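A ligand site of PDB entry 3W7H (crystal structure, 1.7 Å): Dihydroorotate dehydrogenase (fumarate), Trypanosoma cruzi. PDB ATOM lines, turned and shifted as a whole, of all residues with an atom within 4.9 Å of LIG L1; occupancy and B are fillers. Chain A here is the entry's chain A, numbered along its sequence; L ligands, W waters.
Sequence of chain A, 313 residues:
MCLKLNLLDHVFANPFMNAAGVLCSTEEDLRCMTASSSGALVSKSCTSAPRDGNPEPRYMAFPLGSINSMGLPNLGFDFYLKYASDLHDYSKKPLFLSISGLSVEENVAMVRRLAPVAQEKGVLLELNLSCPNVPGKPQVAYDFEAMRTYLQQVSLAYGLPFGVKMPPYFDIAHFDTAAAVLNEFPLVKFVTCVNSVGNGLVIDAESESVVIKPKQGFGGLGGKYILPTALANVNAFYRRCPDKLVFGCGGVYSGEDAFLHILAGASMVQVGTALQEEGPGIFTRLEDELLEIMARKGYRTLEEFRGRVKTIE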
ATOM      1  N   ALA A  19      14.399 -19.227 -16.290  1.00  0.00           N
ATOM      2  CA  ALA A  19      13.796 -18.563 -15.149  1.00  0.00           C
ATOM      3  C   ALA A  19      13.623 -17.086 -15.444  1.00  0.00           C
ATOM      4  O   ALA A  19      14.426 -16.475 -16.121  1.00  0.00           O
ATOM      5  CB  ALA A  19      14.720 -18.795 -13.930  1.00  0.00           C
ATOM      6  N   ALA A  20      12.559 -16.453 -14.966  1.00  0.00           N
ATOM      7  CA  ALA A  20      12.367 -15.100 -15.217  1.00  0.00           C
ATOM      8  C   ALA A  20      13.564 -14.277 -14.730  1.00  0.00           C
ATOM      9  O   ALA A  20      14.158 -14.572 -13.702  1.00  0.00           O
ATOM     10  CB  ALA A  20      11.064 -14.552 -14.512  1.00  0.00           C
ATOM     11  N   GLY A  21      13.969 -13.313 -15.546  1.00  0.00           N
ATOM     12  CA  GLY A  21      15.041 -12.479 -15.236  1.00  0.00           C
ATOM     13  C   GLY A  21      16.284 -12.833 -16.032  1.00  0.00           C
ATOM     14  O   GLY A  21      17.194 -11.989 -16.183  1.00  0.00           O
ATOM     15  N   VAL A  22      16.405 -14.094 -16.427  1.00  0.00           N
ATOM     16  CA  VAL A  22      17.641 -14.516 -17.104  1.00  0.00           C
ATOM     17  C   VAL A  22      17.392 -14.645 -18.607  1.00  0.00           C
ATOM     18  O   VAL A  22      16.507 -15.301 -18.990  1.00  0.00           O
ATOM     19  CB  VAL A  22      18.116 -15.859 -16.515  1.00  0.00           C
ATOM     20  CG1 VAL A  22      19.326 -16.404 -17.226  1.00  0.00           C
ATOM     21  CG2 VAL A  22      18.362 -15.678 -15.046  1.00  0.00           C
ATOM     22  N   LYS A  44      11.249 -11.109 -18.775  1.00  0.00           N
ATOM     23  CA  LYS A  44      11.653 -10.430 -17.607  1.00  0.00           C
ATOM     24  C   LYS A  44      10.465  -9.829 -16.913  1.00  0.00           C
ATOM     25  O   LYS A  44       9.674  -9.145 -17.534  1.00  0.00           O
ATOM     26  CB  LYS A  44      12.588  -9.358 -17.979  1.00  0.00           C
ATOM     27  CG  LYS A  44      13.000  -8.452 -16.865  1.00  0.00           C
ATOM     28  CD  LYS A  44      13.777  -9.030 -15.713  1.00  0.00           C
ATOM     29  CE  LYS A  44      13.829  -8.145 -14.464  1.00  0.00           C
ATOM     30  NZ  LYS A  44      14.677  -8.736 -13.311  1.00  0.00           N
ATOM     31  N   SER A  45      10.390 -10.018 -15.588  1.00  0.00           N
ATOM     32  CA  SER A  45       9.338  -9.422 -14.744  1.00  0.00           C
ATOM     33  C   SER A  45       9.322  -7.944 -15.061  1.00  0.00           C
ATOM     34  O   SER A  45      10.343  -7.298 -15.051  1.00  0.00           O
ATOM     35  CB  SER A  45       9.598  -9.605 -13.317  1.00  0.00           C
ATOM     36  OG  SER A  45       9.353 -10.939 -12.968  1.00  0.00           O
ATOM     37  N   TYR A  59      24.911  -8.343 -10.031  1.00  0.00           N
ATOM     38  CA  TYR A  59      24.899  -9.773 -10.183  1.00  0.00           C
ATOM     39  C   TYR A  59      26.271 -10.306 -10.149  1.00  0.00           C
ATOM     40  O   TYR A  59      27.143  -9.799 -10.893  1.00  0.00           O
ATOM     41  CB  TYR A  59      24.241 -10.173 -11.524  1.00  0.00           C
ATOM     42  CG  TYR A  59      24.353 -11.671 -11.860  1.00  0.00           C
ATOM     43  CD1 TYR A  59      23.447 -12.623 -11.401  1.00  0.00           C
ATOM     44  CD2 TYR A  59      25.451 -12.167 -12.567  1.00  0.00           C
ATOM     45  CE1 TYR A  59      23.548 -13.973 -11.656  1.00  0.00           C
ATOM     46  CE2 TYR A  59      25.582 -13.532 -12.800  1.00  0.00           C
ATOM     47  CZ  TYR A  59      24.646 -14.448 -12.427  1.00  0.00           C
ATOM     48  OH  TYR A  59      24.778 -15.818 -12.742  1.00  0.00           O
ATOM     49  N   SER A  66      24.793 -17.950  -7.437  1.00  0.00           N
ATOM     50  CA  SER A  66      24.818 -16.554  -7.779  1.00  0.00           C
ATOM     51  C   SER A  66      24.118 -15.739  -6.638  1.00  0.00           C
ATOM     52  O   SER A  66      23.355 -16.264  -5.868  1.00  0.00           O
ATOM     53  CB  SER A  66      24.084 -16.285  -9.106  1.00  0.00           C
ATOM     54  OG  SER A  66      22.671 -16.552  -8.940  1.00  0.00           O
ATOM     55  N   ASN A  68      22.150 -11.723  -6.511  1.00  0.00           N
ATOM     56  CA  ASN A  68      21.758 -10.577  -7.275  1.00  0.00           C
ATOM     57  C   ASN A  68      20.891  -9.617  -6.515  1.00  0.00           C
ATOM     58  O   ASN A  68      20.053 -10.026  -5.678  1.00  0.00           O
ATOM     59  CB  ASN A  68      21.045 -11.008  -8.569  1.00  0.00           C
ATOM     60  CG  ASN A  68      19.554 -11.239  -8.353  1.00  0.00           C
ATOM     61  OD1 ASN A  68      18.752 -10.250  -8.409  1.00  0.00           O
ATOM     62  ND2 ASN A  68      19.139 -12.453  -8.233  1.00  0.00           N
ATOM     63  N   MET A  70      19.225  -7.029  -8.703  1.00  0.00           N
ATOM     64  CA  MET A  70      19.122  -6.351  -9.972  1.00  0.00           C
ATOM     65  C   MET A  70      18.199  -5.105  -9.847  1.00  0.00           C
ATOM     66  O   MET A  70      18.456  -4.092 -10.478  1.00  0.00           O
ATOM     67  CB  MET A  70      18.537  -7.247 -10.973  1.00  0.00           C
ATOM     68  CG  MET A  70      19.172  -8.559 -11.281  1.00  0.00           C
ATOM     69  SD  MET A  70      20.839  -8.380 -11.831  1.00  0.00           S
ATOM     70  CE  MET A  70      20.727  -7.785 -13.429  1.00  0.00           C
ATOM     71  N   LEU A  72      14.861  -4.957 -10.647  1.00  0.00           N
ATOM     72  CA  LEU A  72      13.850  -5.006 -11.653  1.00  0.00           C
ATOM     73  C   LEU A  72      14.151  -4.093 -12.816  1.00  0.00           C
ATOM     74  O   LEU A  72      13.273  -3.369 -13.381  1.00  0.00           O
ATOM     75  CB  LEU A  72      12.461  -4.682 -11.011  1.00  0.00           C
ATOM     76  CG  LEU A  72      11.187  -5.333 -11.399  1.00  0.00           C
ATOM     77  CD1 LEU A  72      11.246  -6.804 -11.786  1.00  0.00           C
ATOM     78  CD2 LEU A  72      10.193  -5.070 -10.205  1.00  0.00           C
ATOM     79  N   SER A  98       6.039 -12.460 -17.485  1.00  0.00           N
ATOM     80  CA  SER A  98       6.081 -12.242 -16.025  1.00  0.00           C
ATOM     81  C   SER A  98       5.848 -10.800 -15.644  1.00  0.00           C
ATOM     82  O   SER A  98       6.383  -9.915 -16.314  1.00  0.00           O
ATOM     83  CB  SER A  98       7.391 -12.668 -15.434  1.00  0.00           C
ATOM     84  OG  SER A  98       7.466 -12.319 -14.020  1.00  0.00           O
ATOM     85  N   GLU A 126       2.659 -15.112 -15.651  1.00  0.00           N
ATOM     86  CA  GLU A 126       3.319 -15.482 -14.395  1.00  0.00           C
ATOM     87  C   GLU A 126       3.417 -14.218 -13.521  1.00  0.00           C
ATOM     88  O   GLU A 126       4.134 -13.262 -13.823  1.00  0.00           O
ATOM     89  CB  GLU A 126       4.725 -16.160 -14.602  1.00  0.00           C
ATOM     90  CG  GLU A 126       5.342 -16.657 -13.295  1.00  0.00           C
ATOM     91  CD  GLU A 126       6.688 -17.409 -13.488  1.00  0.00           C
ATOM     92  OE1 GLU A 126       7.723 -16.712 -13.527  1.00  0.00           O
ATOM     93  OE2 GLU A 126       6.778 -18.672 -13.607  1.00  0.00           O
ATOM     94  N   ASN A 128       4.664 -12.400 -10.338  1.00  0.00           N
ATOM     95  CA  ASN A 128       5.712 -12.516  -9.373  1.00  0.00           C
ATOM     96  C   ASN A 128       5.290 -11.929  -8.047  1.00  0.00           C
ATOM     97  O   ASN A 128       5.141 -10.757  -7.920  1.00  0.00           O
ATOM     98  CB  ASN A 128       6.916 -11.739  -9.882  1.00  0.00           C
ATOM     99  CG  ASN A 128       8.104 -11.862  -8.977  1.00  0.00           C
ATOM    100  OD1 ASN A 128       8.106 -12.536  -8.081  1.00  0.00           O
ATOM    101  ND2 ASN A 128       9.109 -11.146  -9.304  1.00  0.00           N
ATOM    102  N   LYS A 165       4.676 -16.821  -9.182  1.00  0.00           N
ATOM    103  CA  LYS A 165       6.075 -17.130  -8.815  1.00  0.00           C
ATOM    104  C   LYS A 165       6.242 -16.829  -7.333  1.00  0.00           C
ATOM    105  O   LYS A 165       5.966 -15.729  -6.845  1.00  0.00           O
ATOM    106  CB  LYS A 165       7.021 -16.287  -9.648  1.00  0.00           C
ATOM    107  CG  LYS A 165       8.499 -16.385  -9.263  1.00  0.00           C
ATOM    108  CD  LYS A 165       9.134 -17.642  -9.887  1.00  0.00           C
ATOM    109  CE  LYS A 165      10.617 -17.654  -9.862  1.00  0.00           C
ATOM    110  NZ  LYS A 165      11.195 -16.789 -10.837  1.00  0.00           N
ATOM    111  N   VAL A 194      11.100 -22.087  -6.953  1.00  0.00           N
ATOM    112  CA  VAL A 194      11.061 -20.899  -6.151  1.00  0.00           C
ATOM    113  C   VAL A 194      11.829 -19.755  -6.788  1.00  0.00           C
ATOM    114  O   VAL A 194      12.654 -19.946  -7.595  1.00  0.00           O
ATOM    115  CB  VAL A 194      11.725 -21.129  -4.782  1.00  0.00           C
ATOM    116  CG1 VAL A 194      10.985 -22.199  -4.036  1.00  0.00           C
ATOM    117  CG2 VAL A 194      13.136 -21.601  -5.003  1.00  0.00           C
ATOM    118  N   ASN A 195      11.522 -18.570  -6.327  1.00  0.00           N
ATOM    119  CA  ASN A 195      12.395 -17.411  -6.560  1.00  0.00           C
ATOM    120  C   ASN A 195      13.664 -17.529  -5.698  1.00  0.00           C
ATOM    121  O   ASN A 195      13.832 -18.457  -5.022  1.00  0.00           O
ATOM    122  CB  ASN A 195      11.614 -16.103  -6.210  1.00  0.00           C
ATOM    123  CG  ASN A 195      12.022 -14.920  -7.057  1.00  0.00           C
ATOM    124  OD1 ASN A 195      13.134 -14.651  -7.164  1.00  0.00           O
ATOM    125  ND2 ASN A 195      11.057 -14.220  -7.593  1.00  0.00           N
ATOM    126  N   SER A 196      14.532 -16.530  -5.786  1.00  0.00           N
ATOM    127  CA  SER A 196      15.813 -16.637  -5.134  1.00  0.00           C
ATOM    128  C   SER A 196      15.663 -16.663  -3.610  1.00  0.00           C
ATOM    129  O   SER A 196      14.676 -16.243  -3.102  1.00  0.00           O
ATOM    130  CB  SER A 196      16.684 -15.482  -5.586  1.00  0.00           C
ATOM    131  OG  SER A 196      16.039 -14.316  -5.439  1.00  0.00           O
ATOM    132  N   GLY A 222      20.803 -17.821  -5.904  1.00  0.00           N
ATOM    133  CA  GLY A 222      20.415 -18.884  -6.761  1.00  0.00           C
ATOM    134  C   GLY A 222      21.521 -19.906  -6.947  1.00  0.00           C
ATOM    135  O   GLY A 222      22.659 -19.705  -6.463  1.00  0.00           O
ATOM    136  N   GLY A 223      21.190 -20.965  -7.646  1.00  0.00           N
ATOM    137  CA  GLY A 223      22.129 -21.951  -8.040  1.00  0.00           C
ATOM    138  C   GLY A 223      22.266 -23.136  -7.056  1.00  0.00           C
ATOM    139  O   GLY A 223      21.304 -23.533  -6.396  1.00  0.00           O
ATOM    140  N   ILE A 226      20.749 -23.526  -3.507  1.00  0.00           N
ATOM    141  CA  ILE A 226      19.332 -23.491  -3.224  1.00  0.00           C
ATOM    142  C   ILE A 226      18.551 -24.765  -3.666  1.00  0.00           C
ATOM    143  O   ILE A 226      17.352 -24.812  -3.461  1.00  0.00           O
ATOM    144  CB  ILE A 226      18.658 -22.237  -3.714  1.00  0.00           C
ATOM    145  CG1 ILE A 226      18.398 -22.231  -5.214  1.00  0.00           C
ATOM    146  CG2 ILE A 226      19.421 -21.004  -3.307  1.00  0.00           C
ATOM    147  CD1 ILE A 226      17.301 -21.240  -5.574  1.00  0.00           C
ATOM    148  N   CYS A 249      11.852 -24.365 -10.030  1.00  0.00           N
ATOM    149  CA  CYS A 249      12.948 -23.433 -10.323  1.00  0.00           C
ATOM    150  C   CYS A 249      13.887 -23.439  -9.121  1.00  0.00           C
ATOM    151  O   CYS A 249      13.463 -23.333  -7.992  1.00  0.00           O
ATOM    152  CB  CYS A 249      12.399 -22.046 -10.578  1.00  0.00           C
ATOM    153  SG  CYS A 249      13.619 -20.865 -11.143  1.00  0.00           S
ATOM    154  N   GLY A 250      15.154 -23.621  -9.364  1.00  0.00           N
ATOM    155  CA  GLY A 250      16.223 -23.476  -8.395  1.00  0.00           C
ATOM    156  C   GLY A 250      17.225 -24.596  -8.464  1.00  0.00           C
ATOM    157  O   GLY A 250      16.934 -25.749  -8.282  1.00  0.00           O
ATOM    158  N   GLY A 251      18.445 -24.165  -8.678  1.00  0.00           N
ATOM    159  CA  GLY A 251      19.554 -25.142  -8.638  1.00  0.00           C
ATOM    160  C   GLY A 251      19.652 -26.082  -9.754  1.00  0.00           C
ATOM    161  O   GLY A 251      20.355 -27.056  -9.552  1.00  0.00           O
ATOM    162  N   VAL A 252      19.010 -25.863 -10.901  1.00  0.00           N
ATOM    163  CA  VAL A 252      19.131 -26.829 -11.955  1.00  0.00           C
ATOM    164  C   VAL A 252      20.396 -26.547 -12.778  1.00  0.00           C
ATOM    165  O   VAL A 252      20.431 -25.508 -13.440  1.00  0.00           O
ATOM    166  CB  VAL A 252      17.852 -26.867 -12.878  1.00  0.00           C
ATOM    167  CG1 VAL A 252      18.045 -27.782 -14.056  1.00  0.00           C
ATOM    168  CG2 VAL A 252      16.632 -27.270 -12.080  1.00  0.00           C
ATOM    169  N   GLN A 270      12.517 -24.611 -14.650  1.00  0.00           N
ATOM    170  CA  GLN A 270      13.099 -23.343 -15.130  1.00  0.00           C
ATOM    171  C   GLN A 270      14.602 -23.348 -14.683  1.00  0.00           C
ATOM    172  O   GLN A 270      14.960 -23.965 -13.656  1.00  0.00           O
ATOM    173  CB  GLN A 270      12.401 -22.180 -14.410  1.00  0.00           C
ATOM    174  CG  GLN A 270      10.902 -22.231 -14.600  1.00  0.00           C
ATOM    175  CD  GLN A 270      10.229 -20.969 -14.154  1.00  0.00           C
ATOM    176  OE1 GLN A 270      10.740 -20.256 -13.299  1.00  0.00           O
ATOM    177  NE2 GLN A 270       9.081 -20.701 -14.714  1.00  0.00           N
ATOM    178  N   VAL A 271      15.409 -22.622 -15.442  1.00  0.00           N
ATOM    179  CA  VAL A 271      16.837 -22.599 -15.303  1.00  0.00           C
ATOM    180  C   VAL A 271      17.263 -21.146 -15.305  1.00  0.00           C
ATOM    181  O   VAL A 271      17.076 -20.414 -16.264  1.00  0.00           O
ATOM    182  CB  VAL A 271      17.512 -23.363 -16.446  1.00  0.00           C
ATOM    183  CG1 VAL A 271      18.962 -23.454 -16.137  1.00  0.00           C
ATOM    184  CG2 VAL A 271      16.870 -24.709 -16.670  1.00  0.00           C
ATOM    185  N   GLY A 272      17.808 -20.723 -14.156  1.00  0.00           N
ATOM    186  CA  GLY A 272      18.215 -19.296 -13.880  1.00  0.00           C
ATOM    187  C   GLY A 272      19.755 -19.272 -13.990  1.00  0.00           C
ATOM    188  O   GLY A 272      20.355 -19.105 -15.043  1.00  0.00           O
ATOM    189  N   THR A 273      20.406 -19.316 -12.846  1.00  0.00           N
ATOM    190  CA  THR A 273      21.855 -19.165 -12.685  1.00  0.00           C
ATOM    191  C   THR A 273      22.643 -19.986 -13.691  1.00  0.00           C
ATOM    192  O   THR A 273      23.502 -19.481 -14.367  1.00  0.00           O
ATOM    193  CB  THR A 273      22.281 -19.559 -11.276  1.00  0.00           C
ATOM    194  OG1 THR A 273      21.680 -18.644 -10.307  1.00  0.00           O
ATOM    195  CG2 THR A 273      23.766 -19.407 -11.120  1.00  0.00           C
ATOM    196  N   ALA A 274      22.280 -21.245 -13.857  1.00  0.00           N
ATOM    197  CA  ALA A 274      23.103 -22.053 -14.772  1.00  0.00           C
ATOM    198  C   ALA A 274      22.996 -21.603 -16.199  1.00  0.00           C
ATOM    199  O   ALA A 274      23.943 -21.743 -16.979  1.00  0.00           O
ATOM    200  CB  ALA A 274      22.650 -23.482 -14.662  1.00  0.00           C
HETATM  201  N1  LIG L   1      12.624 -14.003 -10.692  1.00  0.00           N
HETATM  202  C1  LIG L   1      11.484 -13.365 -11.135  1.00  0.00           C
HETATM  203  O1  LIG L   1      10.419 -13.967 -10.934  1.00  0.00           O
HETATM  204  N2  LIG L   1      11.502 -12.227 -11.855  1.00  0.00           N
HETATM  205  C2  LIG L   1      12.674 -11.631 -12.242  1.00  0.00           C
HETATM  206  O2  LIG L   1      12.718 -10.557 -12.941  1.00  0.00           O
HETATM  207  C3  LIG L   1      13.900 -12.189 -11.796  1.00  0.00           C
HETATM  208  N3  LIG L   1      15.091 -11.635 -12.111  1.00  0.00           N
HETATM  209  C4  LIG L   1      16.277 -12.331 -11.861  1.00  0.00           C
HETATM  210  C5  LIG L   1      17.484 -11.820 -12.392  1.00  0.00           C
HETATM  211  C6  LIG L   1      18.644 -12.488 -12.105  1.00  0.00           C
HETATM  212  C7  LIG L   1      19.947 -12.025 -12.626  1.00  0.00           C
HETATM  213  C8  LIG L   1      18.582 -13.757 -11.400  1.00  0.00           C
HETATM  214  C9  LIG L   1      19.808 -14.513 -11.157  1.00  0.00           C
HETATM  215  C10 LIG L   1      17.377 -14.262 -10.915  1.00  0.00           C
HETATM  216  C11 LIG L   1      16.227 -13.563 -11.128  1.00  0.00           C
HETATM  217  N4  LIG L   1      14.976 -14.043 -10.657  1.00  0.00           N
HETATM  218  C12 LIG L   1      13.806 -13.455 -11.038  1.00  0.00           C
HETATM  219  C13 LIG L   1      14.903 -15.325  -9.937  1.00  0.00           C
HETATM  220  C14 LIG L   1      15.036 -16.499 -10.880  1.00  0.00           C
HETATM  221  O3  LIG L   1      13.892 -16.515 -11.705  1.00  0.00           O
HETATM  222  C15 LIG L   1      15.058 -17.781 -10.129  1.00  0.00           C
HETATM  223  O4  LIG L   1      13.836 -17.914  -9.396  1.00  0.00           O
HETATM  224  C16 LIG L   1      16.245 -17.884  -9.136  1.00  0.00           C
HETATM  225  O5  LIG L   1      17.449 -17.371  -9.762  1.00  0.00           O
HETATM  226  C17 LIG L   1      16.492 -19.376  -8.745  1.00  0.00           C
HETATM  227  O6  LIG L   1      16.784 -20.246  -9.820  1.00  0.00           O
HETATM  228  P1  LIG L   1      18.313 -20.693 -10.152  1.00  0.00           P
HETATM  229  O7  LIG L   1      18.247 -21.522 -11.413  1.00  0.00           O
HETATM  230  O8  LIG L   1      18.787 -21.419  -8.954  1.00  0.00           O
HETATM  231  O9  LIG L   1      19.079 -19.396 -10.371  1.00  0.00           O
HETATM  232  O1  LG2 L   2      16.290  -7.950  -8.534  1.00  0.00           O
HETATM  233  C1  LG2 L   2      15.428  -8.379  -9.315  1.00  0.00           C
HETATM  234  O2  LG2 L   2      15.066  -7.787 -10.327  1.00  0.00           O
HETATM  235  C2  LG2 L   2      14.821  -9.704  -8.955  1.00  0.00           C
HETATM  236  N1  LG2 L   2      15.797 -10.656  -8.551  1.00  0.00           N
HETATM  237  C3  LG2 L   2      15.439 -11.918  -8.180  1.00  0.00           C
HETATM  238  O3  LG2 L   2      16.295 -12.716  -7.799  1.00  0.00           O
HETATM  239  N2  LG2 L   2      14.085 -12.187  -8.174  1.00  0.00           N
HETATM  240  C4  LG2 L   2      13.064 -11.249  -8.422  1.00  0.00           C
HETATM  241  O4  LG2 L   2      11.871 -11.592  -8.423  1.00  0.00           O
HETATM  242  C5  LG2 L   2      13.495  -9.975  -8.902  1.00  0.00           C
HETATM  243  C6  LG2 L   2      12.524  -9.006  -9.180  1.00  0.00           C
HETATM  244  C7  LG2 L   2      11.802  -8.497  -7.828  1.00  0.00           C
HETATM  245  C8  LG2 L   2      12.622  -7.515  -7.190  1.00  0.00           C
HETATM  246  C9  LG2 L   2      12.358  -6.143  -7.319  1.00  0.00           C
HETATM  247  C10 LG2 L   2      13.255  -5.204  -6.685  1.00  0.00           C
HETATM  248  C11 LG2 L   2      13.027  -3.823  -6.806  1.00  0.00           C
HETATM  249  C12 LG2 L   2      13.908  -2.925  -6.225  1.00  0.00           C
HETATM  250  C13 LG2 L   2      15.008  -3.324  -5.467  1.00  0.00           C
HETATM  251  C14 LG2 L   2      15.219  -4.686  -5.284  1.00  0.00           C
HETATM  252  C15 LG2 L   2      14.356  -5.610  -5.939  1.00  0.00           C
HETATM  253  C16 LG2 L   2      14.568  -6.975  -5.797  1.00  0.00           C
HETATM  254  C17 LG2 L   2      13.709  -7.902  -6.399  1.00  0.00           C
HETATM  255  O   HOH W   1      17.248  -9.262 -14.738  1.00  0.00           O
HETATM  256  O   HOH W   2       8.028 -14.274 -12.386  1.00  0.00           O
HETATM  257  O   HOH W   3      20.444 -22.761 -12.302  1.00  0.00           O
HETATM  258  O   HOH W   4      18.493 -16.076  -7.930  1.00  0.00           O
HETATM  259  O   HOH W   5      16.907 -23.809 -11.649  1.00  0.00           O
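The backbone NH of Gly 223 sits at hydrogen-bond distance from an oxygen (O8) of LIG L1 (2.8 Å). N2 of LIG L1 lies within hydrogen-bond range of OG of Ser 45 (2.7 Å). The backbone NH of Gly 272 is in hydrogen-bond range of an oxygen (O7) of LIG L1 (2.9 Å). The side-chain amide nitrogen (ND2) of Asn 68 sits at hydrogen-bond distance from an oxygen (O3) of LG2 L2, at 2.9 Å. The side-chain hydroxyl (OG1) of Thr 273 is in hydrogen-bond range of an oxygen (O9) of LIG L1 (2.7 Å). OD1 of Asn 195 lies within hydrogen-bond range of N2 of LG2 L2, at 2.8 Å. The side-chain amino group (NZ) of Lys 44 lies within hydrogen-bond range of an oxygen (O2) of LIG L1 (2.7 Å). The side-chain amino group (NZ) of Lys 44 is in salt-bridge range of an oxygen (O2) of LG2 L2 (3.2 Å). The backbone NH (N) of Gly 251 is in hydrogen-bond range of an oxygen (O8) of LIG L1, at 2.8 Å. The backbone NH (N) of Thr 273 sits at hydrogen-bond distance from an oxygen (O9) of LIG L1, at 2.8 Å. The side-chain hydroxyl (OG) of Ser 196 sits at hydrogen-bond distance from an oxygen (O3) of LG2 L2 (2.9 Å). O4 of LIG L1 sits at hydrogen-bond distance from O of Val 194 (3.0 Å). The side-chain amino group (NZ) of Lys 165 is in hydrogen-bond range of an oxygen (O3) of LIG L1 (2.8 Å). SG of Cys 249 sits at hydrogen-bond distance from O4 of LIG L1 (3.4 Å). N of Leu 72 is in hydrogen-bond range of O2 of LG2 L2 (2.9 Å). The backbone NH (N) of Met 70 lies within hydrogen-bond range of an oxygen (O1) of LG2 L2. The backbone carbonyl oxygen (O) of Ala 20 is in hydrogen-bond range of an oxygen (O3) of LIG L1, 2.8 Å away. An oxygen (O4) of LG2 L2 is in hydrogen-bond range of the side-chain amide nitrogen of Asn 128, 2.9 Å away. ND2 of Asn 195 lies within hydrogen-bond range of O1 of LIG L1 (3.4 Å).
A nitrogen (N1) of LIG L1 sits close to a nitrogen (N2) of LG2 L2, 3.4 Å away.
OG of Ser 45 lies within hydrogen-bond range of OG of Ser 98 (2.6 Å). OD1 of Asn 195 is in hydrogen-bond range of OG of Ser 196. The side-chain amide oxygen of Gln 270 is in hydrogen-bond range of the side-chain sulfur of Cys 249, at 3.6 Å. N of Ser 66 lies within hydrogen-bond range of O of Gly 222 (2.9 Å). OG1 of Thr 273 lies within hydrogen-bond range of OG of Ser 66, at 2.7 Å. The backbone NH (N) of Val 194 lies within hydrogen-bond range of the backbone carbonyl oxygen (O) of Cys 249, 2.9 Å away. N of Ala 19 is in hydrogen-bond range of O of Val 271 (2.9 Å). The side-chain amide nitrogen of Asn 195 is in hydrogen-bond range of the side-chain amide oxygen of Asn 128, at 3.4 Å.
Residues that only touch LIG L1: Ala 19 (3.3 Å), Gly 21 (3.2 Å), Tyr 59 (3.8 Å), Asn 68 (3.5 Å), Met 70 (3.8 Å), Asn 128 (3.5 Å), Ser 196 (3.9 Å), Gly 222 (3.7 Å), Ile 226 (3.7 Å) and Gly 250 (3.3 Å). Hydrophobic or aromatic side chains that line LIG L1: Ala 19, Ala 20, Tyr 59, Met 70 and Ile 226. 21 residues have an atom within 4 Å of LIG L1: Ala 19, Ala 20, Gly 21, Lys 44, Ser 45, Tyr 59, Asn 68, Met 70, Asn 128, Lys 165, Val 194, Asn 195, Ser 196, Gly 222, Gly 223, Ile 226, Cys 249, Gly 250, Gly 251, Gly 272 and Thr 273.
Water W3 lies within hydrogen-bond range of an oxygen (O7) of LIG L1 (2.7 Å), the backbone NH (N) of Ala 274 (2.8 Å), the backbone carbonyl oxygen (O) of Val 252 (3.0 Å) and the backbone NH (N) of Thr 273 (3.5 Å). Water W2 lies within hydrogen-bond range of OG of Ser 98 (2.6 Å), OE1 of Glu 126 (2.7 Å) and O1 of LIG L1 (2.8 Å). Water W1 lies within hydrogen-bond range of NZ of Lys 44 and O of Gly 21.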
